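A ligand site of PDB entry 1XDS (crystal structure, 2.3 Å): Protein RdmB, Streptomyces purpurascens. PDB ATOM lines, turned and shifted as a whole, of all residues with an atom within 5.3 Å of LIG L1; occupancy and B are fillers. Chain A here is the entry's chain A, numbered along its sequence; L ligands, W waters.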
ATOM      1  N   TRP A 146      17.076 -24.274  26.161  1.00  0.00           N
ATOM      2  CA  TRP A 146      17.651 -25.592  26.431  1.00  0.00           C
ATOM      3  C   TRP A 146      16.706 -26.485  27.185  1.00  0.00           C
ATOM      4  O   TRP A 146      16.714 -27.692  26.994  1.00  0.00           O
ATOM      5  CB  TRP A 146      18.967 -25.474  27.207  1.00  0.00           C
ATOM      6  CG  TRP A 146      19.994 -24.818  26.406  1.00  0.00           C
ATOM      7  CD1 TRP A 146      20.538 -23.604  26.629  1.00  0.00           C
ATOM      8  CD2 TRP A 146      20.570 -25.308  25.188  1.00  0.00           C
ATOM      9  NE1 TRP A 146      21.446 -23.311  25.641  1.00  0.00           N
ATOM     10  CE2 TRP A 146      21.474 -24.336  24.740  1.00  0.00           C
ATOM     11  CE3 TRP A 146      20.404 -26.477  24.433  1.00  0.00           C
ATOM     12  CZ2 TRP A 146      22.220 -24.493  23.572  1.00  0.00           C
ATOM     13  CZ3 TRP A 146      21.131 -26.635  23.288  1.00  0.00           C
ATOM     14  CH2 TRP A 146      22.036 -25.653  22.854  1.00  0.00           C
ATOM     15  N   PHE A 159      17.855 -29.756  15.990  1.00  0.00           N
ATOM     16  CA  PHE A 159      18.921 -28.844  16.360  1.00  0.00           C
ATOM     17  C   PHE A 159      20.298 -29.485  16.235  1.00  0.00           C
ATOM     18  O   PHE A 159      21.256 -28.832  15.830  1.00  0.00           O
ATOM     19  CB  PHE A 159      18.758 -28.311  17.783  1.00  0.00           C
ATOM     20  CG  PHE A 159      19.853 -27.387  18.164  1.00  0.00           C
ATOM     21  CD1 PHE A 159      19.879 -26.098  17.647  1.00  0.00           C
ATOM     22  CD2 PHE A 159      20.907 -27.821  18.941  1.00  0.00           C
ATOM     23  CE1 PHE A 159      20.900 -25.240  17.959  1.00  0.00           C
ATOM     24  CE2 PHE A 159      21.948 -26.969  19.247  1.00  0.00           C
ATOM     25  CZ  PHE A 159      21.950 -25.691  18.762  1.00  0.00           C
ATOM     26  N   ASP A 160      20.389 -30.767  16.598  1.00  0.00           N
ATOM     27  CA  ASP A 160      21.633 -31.524  16.491  1.00  0.00           C
ATOM     28  C   ASP A 160      21.976 -31.727  15.027  1.00  0.00           C
ATOM     29  O   ASP A 160      23.147 -31.652  14.642  1.00  0.00           O
ATOM     30  CB  ASP A 160      21.526 -32.903  17.179  1.00  0.00           C
ATOM     31  CG  ASP A 160      21.390 -32.806  18.713  1.00  0.00           C
ATOM     32  OD1 ASP A 160      20.898 -33.780  19.329  1.00  0.00           O
ATOM     33  OD2 ASP A 160      21.737 -31.807  19.390  1.00  0.00           O
ATOM     34  N   MET A 163      23.410 -28.225  13.524  1.00  0.00           N
ATOM     35  CA  MET A 163      24.790 -27.919  13.910  1.00  0.00           C
ATOM     36  C   MET A 163      25.841 -28.904  13.301  1.00  0.00           C
ATOM     37  O   MET A 163      27.015 -28.544  13.240  1.00  0.00           O
ATOM     38  CB  MET A 163      24.943 -27.863  15.453  1.00  0.00           C
ATOM     39  CG  MET A 163      24.354 -26.622  16.191  1.00  0.00           C
ATOM     40  SD  MET A 163      24.516 -24.972  15.393  1.00  0.00           S
ATOM     41  CE  MET A 163      23.004 -24.966  14.540  1.00  0.00           C
ATOM     42  N   ASP A 188      36.293 -32.336  24.174  1.00  0.00           N
ATOM     43  CA  ASP A 188      35.350 -31.405  23.528  1.00  0.00           C
ATOM     44  C   ASP A 188      34.182 -31.191  24.464  1.00  0.00           C
ATOM     45  O   ASP A 188      33.390 -32.103  24.682  1.00  0.00           O
ATOM     46  CB  ASP A 188      34.856 -31.921  22.160  1.00  0.00           C
ATOM     47  CG  ASP A 188      34.235 -30.826  21.304  1.00  0.00           C
ATOM     48  OD1 ASP A 188      33.981 -29.722  21.846  1.00  0.00           O
ATOM     49  OD2 ASP A 188      33.980 -30.948  20.085  1.00  0.00           O
ATOM     50  N   VAL A 189      34.112 -30.002  25.034  1.00  0.00           N
ATOM     51  CA  VAL A 189      33.084 -29.607  25.998  1.00  0.00           C
ATOM     52  C   VAL A 189      31.865 -29.040  25.220  1.00  0.00           C
ATOM     53  O   VAL A 189      31.960 -28.029  24.523  1.00  0.00           O
ATOM     54  CB  VAL A 189      33.699 -28.561  26.979  1.00  0.00           C
ATOM     55  CG1 VAL A 189      32.690 -28.116  28.013  1.00  0.00           C
ATOM     56  CG2 VAL A 189      34.978 -29.121  27.665  1.00  0.00           C
ATOM     57  N   GLY A 190      30.730 -29.703  25.322  1.00  0.00           N
ATOM     58  CA  GLY A 190      29.556 -29.330  24.518  1.00  0.00           C
ATOM     59  C   GLY A 190      29.772 -29.574  23.035  1.00  0.00           C
ATOM     60  O   GLY A 190      29.405 -28.744  22.194  1.00  0.00           O
ATOM     61  N   GLY A 191      30.350 -30.717  22.691  1.00  0.00           N
ATOM     62  CA  GLY A 191      30.766 -30.973  21.327  1.00  0.00           C
ATOM     63  C   GLY A 191      29.685 -31.491  20.386  1.00  0.00           C
ATOM     64  O   GLY A 191      30.017 -32.145  19.422  1.00  0.00           O
ATOM     65  N   GLY A 192      28.421 -31.195  20.666  1.00  0.00           N
ATOM     66  CA  GLY A 192      27.301 -31.637  19.858  1.00  0.00           C
ATOM     67  C   GLY A 192      27.257 -33.144  19.657  1.00  0.00           C
ATOM     68  O   GLY A 192      27.522 -33.935  20.571  1.00  0.00           O
ATOM     69  N   VAL A 212      31.885 -34.306  26.193  1.00  0.00           N
ATOM     70  CA  VAL A 212      30.924 -34.023  27.235  1.00  0.00           C
ATOM     71  C   VAL A 212      29.739 -33.284  26.603  1.00  0.00           C
ATOM     72  O   VAL A 212      29.913 -32.268  25.919  1.00  0.00           O
ATOM     73  CB  VAL A 212      31.538 -33.164  28.349  1.00  0.00           C
ATOM     74  CG1 VAL A 212      30.500 -32.818  29.382  1.00  0.00           C
ATOM     75  CG2 VAL A 212      32.704 -33.917  28.999  1.00  0.00           C
ATOM     76  N   GLU A 213      28.530 -33.808  26.833  1.00  0.00           N
ATOM     77  CA  GLU A 213      27.333 -33.275  26.223  1.00  0.00           C
ATOM     78  C   GLU A 213      26.088 -33.660  27.018  1.00  0.00           C
ATOM     79  O   GLU A 213      26.114 -34.564  27.836  1.00  0.00           O
ATOM     80  CB  GLU A 213      27.199 -33.783  24.775  1.00  0.00           C
ATOM     81  CG  GLU A 213      27.511 -32.746  23.690  1.00  0.00           C
ATOM     82  CD  GLU A 213      26.546 -31.564  23.672  1.00  0.00           C
ATOM     83  OE1 GLU A 213      25.488 -31.659  24.335  1.00  0.00           O
ATOM     84  OE2 GLU A 213      26.842 -30.553  22.989  1.00  0.00           O
ATOM     85  N   LEU A 214      24.987 -32.958  26.782  1.00  0.00           N
ATOM     86  CA  LEU A 214      23.663 -33.372  27.253  1.00  0.00           C
ATOM     87  C   LEU A 214      23.256 -34.765  26.694  1.00  0.00           C
ATOM     88  O   LEU A 214      23.930 -35.313  25.851  1.00  0.00           O
ATOM     89  CB  LEU A 214      22.594 -32.300  26.884  1.00  0.00           C
ATOM     90  CG  LEU A 214      22.834 -30.883  27.432  1.00  0.00           C
ATOM     91  CD1 LEU A 214      21.729 -29.882  27.030  1.00  0.00           C
ATOM     92  CD2 LEU A 214      23.021 -30.929  28.964  1.00  0.00           C
ATOM     93  N   PRO A 217      22.529 -35.150  22.345  1.00  0.00           N
ATOM     94  CA  PRO A 217      23.827 -35.055  21.658  1.00  0.00           C
ATOM     95  C   PRO A 217      24.778 -36.205  22.004  1.00  0.00           C
ATOM     96  O   PRO A 217      25.423 -36.740  21.105  1.00  0.00           O
ATOM     97  CB  PRO A 217      24.385 -33.717  22.132  1.00  0.00           C
ATOM     98  CG  PRO A 217      23.144 -32.869  22.435  1.00  0.00           C
ATOM     99  CD  PRO A 217      22.103 -33.857  22.918  1.00  0.00           C
ATOM    100  N   GLY A 239      26.907 -35.332  30.734  1.00  0.00           N
ATOM    101  CA  GLY A 239      27.230 -34.438  31.817  1.00  0.00           C
ATOM    102  C   GLY A 239      26.854 -33.015  31.483  1.00  0.00           C
ATOM    103  O   GLY A 239      26.351 -32.701  30.400  1.00  0.00           O
ATOM    104  N   ASP A 240      27.137 -32.166  32.446  1.00  0.00           N
ATOM    105  CA  ASP A 240      26.718 -30.773  32.463  1.00  0.00           C
ATOM    106  C   ASP A 240      27.997 -29.987  32.679  1.00  0.00           C
ATOM    107  O   ASP A 240      28.670 -30.158  33.717  1.00  0.00           O
ATOM    108  CB  ASP A 240      25.743 -30.591  33.630  1.00  0.00           C
ATOM    109  CG  ASP A 240      25.286 -29.152  33.842  1.00  0.00           C
ATOM    110  OD1 ASP A 240      25.797 -28.238  33.168  1.00  0.00           O
ATOM    111  OD2 ASP A 240      24.400 -28.848  34.677  1.00  0.00           O
ATOM    112  N   PHE A 241      28.341 -29.112  31.722  1.00  0.00           N
ATOM    113  CA  PHE A 241      29.556 -28.284  31.844  1.00  0.00           C
ATOM    114  C   PHE A 241      29.490 -27.087  32.827  1.00  0.00           C
ATOM    115  O   PHE A 241      30.393 -26.242  32.849  1.00  0.00           O
ATOM    116  CB  PHE A 241      30.080 -27.847  30.458  1.00  0.00           C
ATOM    117  CG  PHE A 241      29.102 -27.082  29.592  1.00  0.00           C
ATOM    118  CD1 PHE A 241      28.177 -26.186  30.128  1.00  0.00           C
ATOM    119  CD2 PHE A 241      29.124 -27.248  28.209  1.00  0.00           C
ATOM    120  CE1 PHE A 241      27.305 -25.476  29.291  1.00  0.00           C
ATOM    121  CE2 PHE A 241      28.254 -26.554  27.377  1.00  0.00           C
ATOM    122  CZ  PHE A 241      27.351 -25.667  27.917  1.00  0.00           C
ATOM    123  N   PHE A 242      28.421 -27.006  33.623  1.00  0.00           N
ATOM    124  CA  PHE A 242      28.356 -26.074  34.764  1.00  0.00           C
ATOM    125  C   PHE A 242      28.849 -26.765  36.040  1.00  0.00           C
ATOM    126  O   PHE A 242      29.156 -26.116  37.031  1.00  0.00           O
ATOM    127  CB  PHE A 242      26.947 -25.500  34.944  1.00  0.00           C
ATOM    128  CG  PHE A 242      26.589 -24.514  33.891  1.00  0.00           C
ATOM    129  CD1 PHE A 242      25.666 -24.830  32.886  1.00  0.00           C
ATOM    130  CD2 PHE A 242      27.194 -23.268  33.859  1.00  0.00           C
ATOM    131  CE1 PHE A 242      25.347 -23.923  31.884  1.00  0.00           C
ATOM    132  CE2 PHE A 242      26.882 -22.354  32.858  1.00  0.00           C
ATOM    133  CZ  PHE A 242      25.947 -22.688  31.859  1.00  0.00           C
ATOM    134  N   SER A 255      33.648 -25.230  21.174  1.00  0.00           N
ATOM    135  CA  SER A 255      33.296 -24.869  19.818  1.00  0.00           C
ATOM    136  C   SER A 255      31.859 -24.380  19.764  1.00  0.00           C
ATOM    137  O   SER A 255      30.931 -25.148  19.937  1.00  0.00           O
ATOM    138  CB  SER A 255      33.457 -26.079  18.914  1.00  0.00           C
ATOM    139  OG  SER A 255      33.461 -25.673  17.579  1.00  0.00           O
ATOM    140  N   PHE A 256      31.694 -23.072  19.583  1.00  0.00           N
ATOM    141  CA  PHE A 256      30.395 -22.430  19.514  1.00  0.00           C
ATOM    142  C   PHE A 256      29.521 -22.750  20.713  1.00  0.00           C
ATOM    143  O   PHE A 256      28.323 -23.060  20.602  1.00  0.00           O
ATOM    144  CB  PHE A 256      29.721 -22.704  18.156  1.00  0.00           C
ATOM    145  CG  PHE A 256      30.346 -21.908  17.043  1.00  0.00           C
ATOM    146  CD1 PHE A 256      31.517 -22.344  16.432  1.00  0.00           C
ATOM    147  CD2 PHE A 256      29.799 -20.688  16.656  1.00  0.00           C
ATOM    148  CE1 PHE A 256      32.128 -21.588  15.424  1.00  0.00           C
ATOM    149  CE2 PHE A 256      30.393 -19.926  15.632  1.00  0.00           C
ATOM    150  CZ  PHE A 256      31.565 -20.376  15.015  1.00  0.00           C
ATOM    151  N   VAL A 257      30.163 -22.653  21.879  1.00  0.00           N
ATOM    152  CA  VAL A 257      29.505 -22.752  23.165  1.00  0.00           C
ATOM    153  C   VAL A 257      29.319 -21.376  23.833  1.00  0.00           C
ATOM    154  O   VAL A 257      28.229 -21.060  24.269  1.00  0.00           O
ATOM    155  CB  VAL A 257      30.311 -23.655  24.067  1.00  0.00           C
ATOM    156  CG1 VAL A 257      29.809 -23.575  25.506  1.00  0.00           C
ATOM    157  CG2 VAL A 257      30.219 -25.083  23.558  1.00  0.00           C
ATOM    158  N   ASN A 260      26.357 -18.789  23.454  1.00  0.00           N
ATOM    159  CA  ASN A 260      25.040 -19.145  24.011  1.00  0.00           C
ATOM    160  C   ASN A 260      24.823 -18.584  25.420  1.00  0.00           C
ATOM    161  O   ASN A 260      23.720 -18.663  25.956  1.00  0.00           O
ATOM    162  CB  ASN A 260      24.902 -20.662  24.166  1.00  0.00           C
ATOM    163  CG  ASN A 260      24.987 -21.431  22.858  1.00  0.00           C
ATOM    164  OD1 ASN A 260      25.085 -22.661  22.872  1.00  0.00           O
ATOM    165  ND2 ASN A 260      24.925 -20.731  21.740  1.00  0.00           N
ATOM    166  N   TRP A 261      25.874 -18.071  26.039  1.00  0.00           N
ATOM    167  CA  TRP A 261      25.816 -17.738  27.459  1.00  0.00           C
ATOM    168  C   TRP A 261      26.162 -16.295  27.765  1.00  0.00           C
ATOM    169  O   TRP A 261      26.833 -15.612  26.991  1.00  0.00           O
ATOM    170  CB  TRP A 261      26.738 -18.681  28.232  1.00  0.00           C
ATOM    171  CG  TRP A 261      26.329 -20.097  28.010  1.00  0.00           C
ATOM    172  CD1 TRP A 261      26.938 -21.001  27.203  1.00  0.00           C
ATOM    173  CD2 TRP A 261      25.179 -20.753  28.549  1.00  0.00           C
ATOM    174  NE1 TRP A 261      26.247 -22.188  27.216  1.00  0.00           N
ATOM    175  CE2 TRP A 261      25.164 -22.069  28.029  1.00  0.00           C
ATOM    176  CE3 TRP A 261      24.132 -20.356  29.408  1.00  0.00           C
ATOM    177  CZ2 TRP A 261      24.173 -23.013  28.360  1.00  0.00           C
ATOM    178  CZ3 TRP A 261      23.136 -21.298  29.752  1.00  0.00           C
ATOM    179  CH2 TRP A 261      23.163 -22.624  29.222  1.00  0.00           C
HETATM  180  N1  LIG L   1      30.637 -27.693  19.819  1.00  0.00           N
HETATM  181  C1  LIG L   1      29.425 -27.780  19.029  1.00  0.00           C
HETATM  182  C2  LIG L   1      29.657 -27.506  17.557  1.00  0.00           C
HETATM  183  O1  LIG L   1      30.448 -26.604  17.206  1.00  0.00           O
HETATM  184  O2  LIG L   1      29.033 -28.192  16.704  1.00  0.00           O
HETATM  185  C3  LIG L   1      28.479 -26.730  19.594  1.00  0.00           C
HETATM  186  C4  LIG L   1      27.036 -27.099  19.366  1.00  0.00           C
HETATM  187  S1  LIG L   1      25.999 -25.987  20.043  1.00  0.00           S
HETATM  188  C5  LIG L   1      26.173 -24.556  19.225  1.00  0.00           C
HETATM  189  C6  LIG L   1      26.070 -25.770  21.712  1.00  0.00           C
HETATM  190  C7  LIG L   1      26.041 -27.128  22.408  1.00  0.00           C
HETATM  191  O3  LIG L   1      26.265 -27.081  23.819  1.00  0.00           O
HETATM  192  C8  LIG L   1      24.766 -27.948  22.201  1.00  0.00           C
HETATM  193  O4  LIG L   1      25.110 -29.087  21.438  1.00  0.00           O
HETATM  194  C9  LIG L   1      24.277 -28.389  23.580  1.00  0.00           C
HETATM  195  O5  LIG L   1      23.975 -29.740  23.767  1.00  0.00           O
HETATM  196  C10 LIG L   1      25.399 -27.978  24.507  1.00  0.00           C
HETATM  197  N2  LIG L   1      25.011 -27.658  25.903  1.00  0.00           N
HETATM  198  C11 LIG L   1      24.123 -26.759  26.391  1.00  0.00           C
HETATM  199  N3  LIG L   1      24.061 -26.789  27.748  1.00  0.00           N
HETATM  200  C12 LIG L   1      24.932 -27.731  28.141  1.00  0.00           C
HETATM  201  C13 LIG L   1      25.384 -28.301  29.318  1.00  0.00           C
HETATM  202  N4  LIG L   1      24.863 -27.828  30.445  1.00  0.00           N
HETATM  203  N5  LIG L   1      26.314 -29.314  29.308  1.00  0.00           N
HETATM  204  C14 LIG L   1      26.844 -29.810  28.182  1.00  0.00           C
HETATM  205  N6  LIG L   1      26.474 -29.354  26.972  1.00  0.00           N
HETATM  206  C15 LIG L   1      25.500 -28.285  26.933  1.00  0.00           C
HETATM  207  O1  LG2 L   2      24.047 -22.296  19.294  1.00  0.00           O
HETATM  208  C1  LG2 L   2      22.981 -21.907  18.750  1.00  0.00           C
HETATM  209  C2  LG2 L   2      21.801 -22.022  19.456  1.00  0.00           C
HETATM  210  C3  LG2 L   2      20.621 -21.585  18.882  1.00  0.00           C
HETATM  211  C4  LG2 L   2      22.968 -21.357  17.472  1.00  0.00           C
HETATM  212  C5  LG2 L   2      21.772 -20.914  16.881  1.00  0.00           C
HETATM  213  C6  LG2 L   2      20.601 -21.042  17.602  1.00  0.00           C
HETATM  214  C7  LG2 L   2      24.236 -21.245  16.721  1.00  0.00           C
HETATM  215  O2  LG2 L   2      25.316 -21.618  17.204  1.00  0.00           O
HETATM  216  C8  LG2 L   2      24.192 -20.661  15.374  1.00  0.00           C
HETATM  217  C9  LG2 L   2      22.877 -20.223  14.808  1.00  0.00           C
HETATM  218  C10 LG2 L   2      21.720 -20.362  15.577  1.00  0.00           C
HETATM  219  O3  LG2 L   2      20.612 -19.964  15.108  1.00  0.00           O
HETATM  220  C11 LG2 L   2      25.340 -20.538  14.644  1.00  0.00           C
HETATM  221  O4  LG2 L   2      26.466 -20.957  15.189  1.00  0.00           O
HETATM  222  C12 LG2 L   2      25.334 -19.993  13.363  1.00  0.00           C
HETATM  223  C13 LG2 L   2      24.117 -19.583  12.816  1.00  0.00           C
HETATM  224  C14 LG2 L   2      22.907 -19.683  13.520  1.00  0.00           C
HETATM  225  C15 LG2 L   2      24.139 -18.974  11.447  1.00  0.00           C
HETATM  226  O5  LG2 L   2      24.021 -17.767  11.492  1.00  0.00           O
HETATM  227  C16 LG2 L   2      25.241 -19.501  10.552  1.00  0.00           C
HETATM  228  O6  LG2 L   2      25.209 -20.943  10.558  1.00  0.00           O
HETATM  229  C17 LG2 L   2      25.197 -19.030   9.086  1.00  0.00           C
HETATM  230  C18 LG2 L   2      24.460 -17.741   8.763  1.00  0.00           C
HETATM  231  C19 LG2 L   2      26.498 -19.092  11.297  1.00  0.00           C
HETATM  232  C20 LG2 L   2      26.616 -19.890  12.595  1.00  0.00           C
HETATM  233  O7  LG2 L   2      27.037 -21.199  12.221  1.00  0.00           O
HETATM  234  C21 LG2 L   2      28.445 -21.422  12.111  1.00  0.00           C
HETATM  235  C22 LG2 L   2      28.874 -22.159  13.367  1.00  0.00           C
HETATM  236  C23 LG2 L   2      28.298 -23.567  13.312  1.00  0.00           C
HETATM  237  N1  LG2 L   2      28.589 -24.168  14.618  1.00  0.00           N
HETATM  238  C24 LG2 L   2      27.704 -24.056  15.541  1.00  0.00           C
HETATM  239  C25 LG2 L   2      29.684 -24.754  14.867  1.00  0.00           C
HETATM  240  O8  LG2 L   2      28.728 -22.185  10.918  1.00  0.00           O
HETATM  241  C26 LG2 L   2      28.219 -23.543  10.915  1.00  0.00           C
HETATM  242  C27 LG2 L   2      28.471 -24.210   9.568  1.00  0.00           C
HETATM  243  C28 LG2 L   2      28.885 -24.259  12.070  1.00  0.00           C
HETATM  244  O9  LG2 L   2      30.300 -24.039  11.912  1.00  0.00           O
HETATM  245  C29 LG2 L   2      31.137 -25.168  11.526  1.00  0.00           C
HETATM  246  C30 LG2 L   2      31.622 -25.303  10.090  1.00  0.00           C
HETATM  247  C31 LG2 L   2      33.147 -25.346  10.053  1.00  0.00           C
HETATM  248  O10 LG2 L   2      33.617 -25.670   8.752  1.00  0.00           O
HETATM  249  O11 LG2 L   2      31.829 -25.899  12.585  1.00  0.00           O
HETATM  250  C32 LG2 L   2      33.265 -25.909  12.476  1.00  0.00           C
HETATM  251  C33 LG2 L   2      33.829 -26.820  13.561  1.00  0.00           C
HETATM  252  C34 LG2 L   2      33.680 -26.350  11.063  1.00  0.00           C
HETATM  253  O12 LG2 L   2      35.104 -26.453  10.920  1.00  0.00           O
HETATM  254  O   HOH W   1      24.299 -30.064  18.980  1.00  0.00           O
HETATM  255  O   HOH W   2      32.544 -27.693  21.806  1.00  0.00           O
HETATM  256  O   HOH W   3      27.914 -30.494  16.558  1.00  0.00           O
HETATM  257  O   HOH W   4      26.159 -24.242  24.903  1.00  0.00           O
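Water W1 bridges O4 of LIG L1 (2.8 Å) and OD2 of Asp 160 (3.1 Å). Water W4 lies within hydrogen-bond range of OD1 of Asn 260 (2.8 Å), O3 of LIG L1 (3.0 Å) and NE1 of Trp 261 (3.1 Å).
O1 of LIG L1 sits at hydrogen-bond distance from OG of Ser 255. The backbone carbonyl oxygen (O) of Gly 190 lies within hydrogen-bond range of a nitrogen (N1) of LIG L1 (2.9 Å). The side-chain carboxylate (OD1) of Asp 240 sits at hydrogen-bond distance from a nitrogen (N4) of LIG L1 (2.9 Å). OE1 of Glu 213 is in hydrogen-bond range of O5 of LIG L1, 2.5 Å away. The backbone carbonyl oxygen (O) of Ser 255 sits at hydrogen-bond distance from a nitrogen (N1) of LIG L1 (2.6 Å). N of Phe 241 is in hydrogen-bond range of N5 of LIG L1 (3.2 Å). ND2 of Asn 260 lies within hydrogen-bond range of O1 of LG2 L2 (3.0 Å).
O of Glu 213 lies within hydrogen-bond range of N of Gly 239 (3.1 Å). N of Gly 190 sits at hydrogen-bond distance from O of Val 212 (2.8 Å). The side-chain carboxylate (OD1) of Asp 240 lies within hydrogen-bond range of the backbone NH (N) of Phe 242 (2.9 Å). N of Gly 192 sits at hydrogen-bond distance from OE2 of Glu 213 (2.9 Å).
The backbone carbonyl oxygen (O) of Phe 256 lies close to a sulfur (S1) of LIG L1 (3.8 Å). Residues that only touch LIG L1: Asn 260 (3.5 Å), Pro 217 (3.5 Å), Leu 214 (3.6 Å), Gly 239 (3.6 Å), Trp 146 (3.6 Å), Gly 191 (3.6 Å), Gly 192 (3.7 Å), Trp 261 (3.8 Å) and Phe 242 (3.9 Å). Hydrophobic or aromatic side chains that line LIG L1: Trp 146, Leu 214, Pro 217, Phe 241, Phe 242 and Trp 261.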
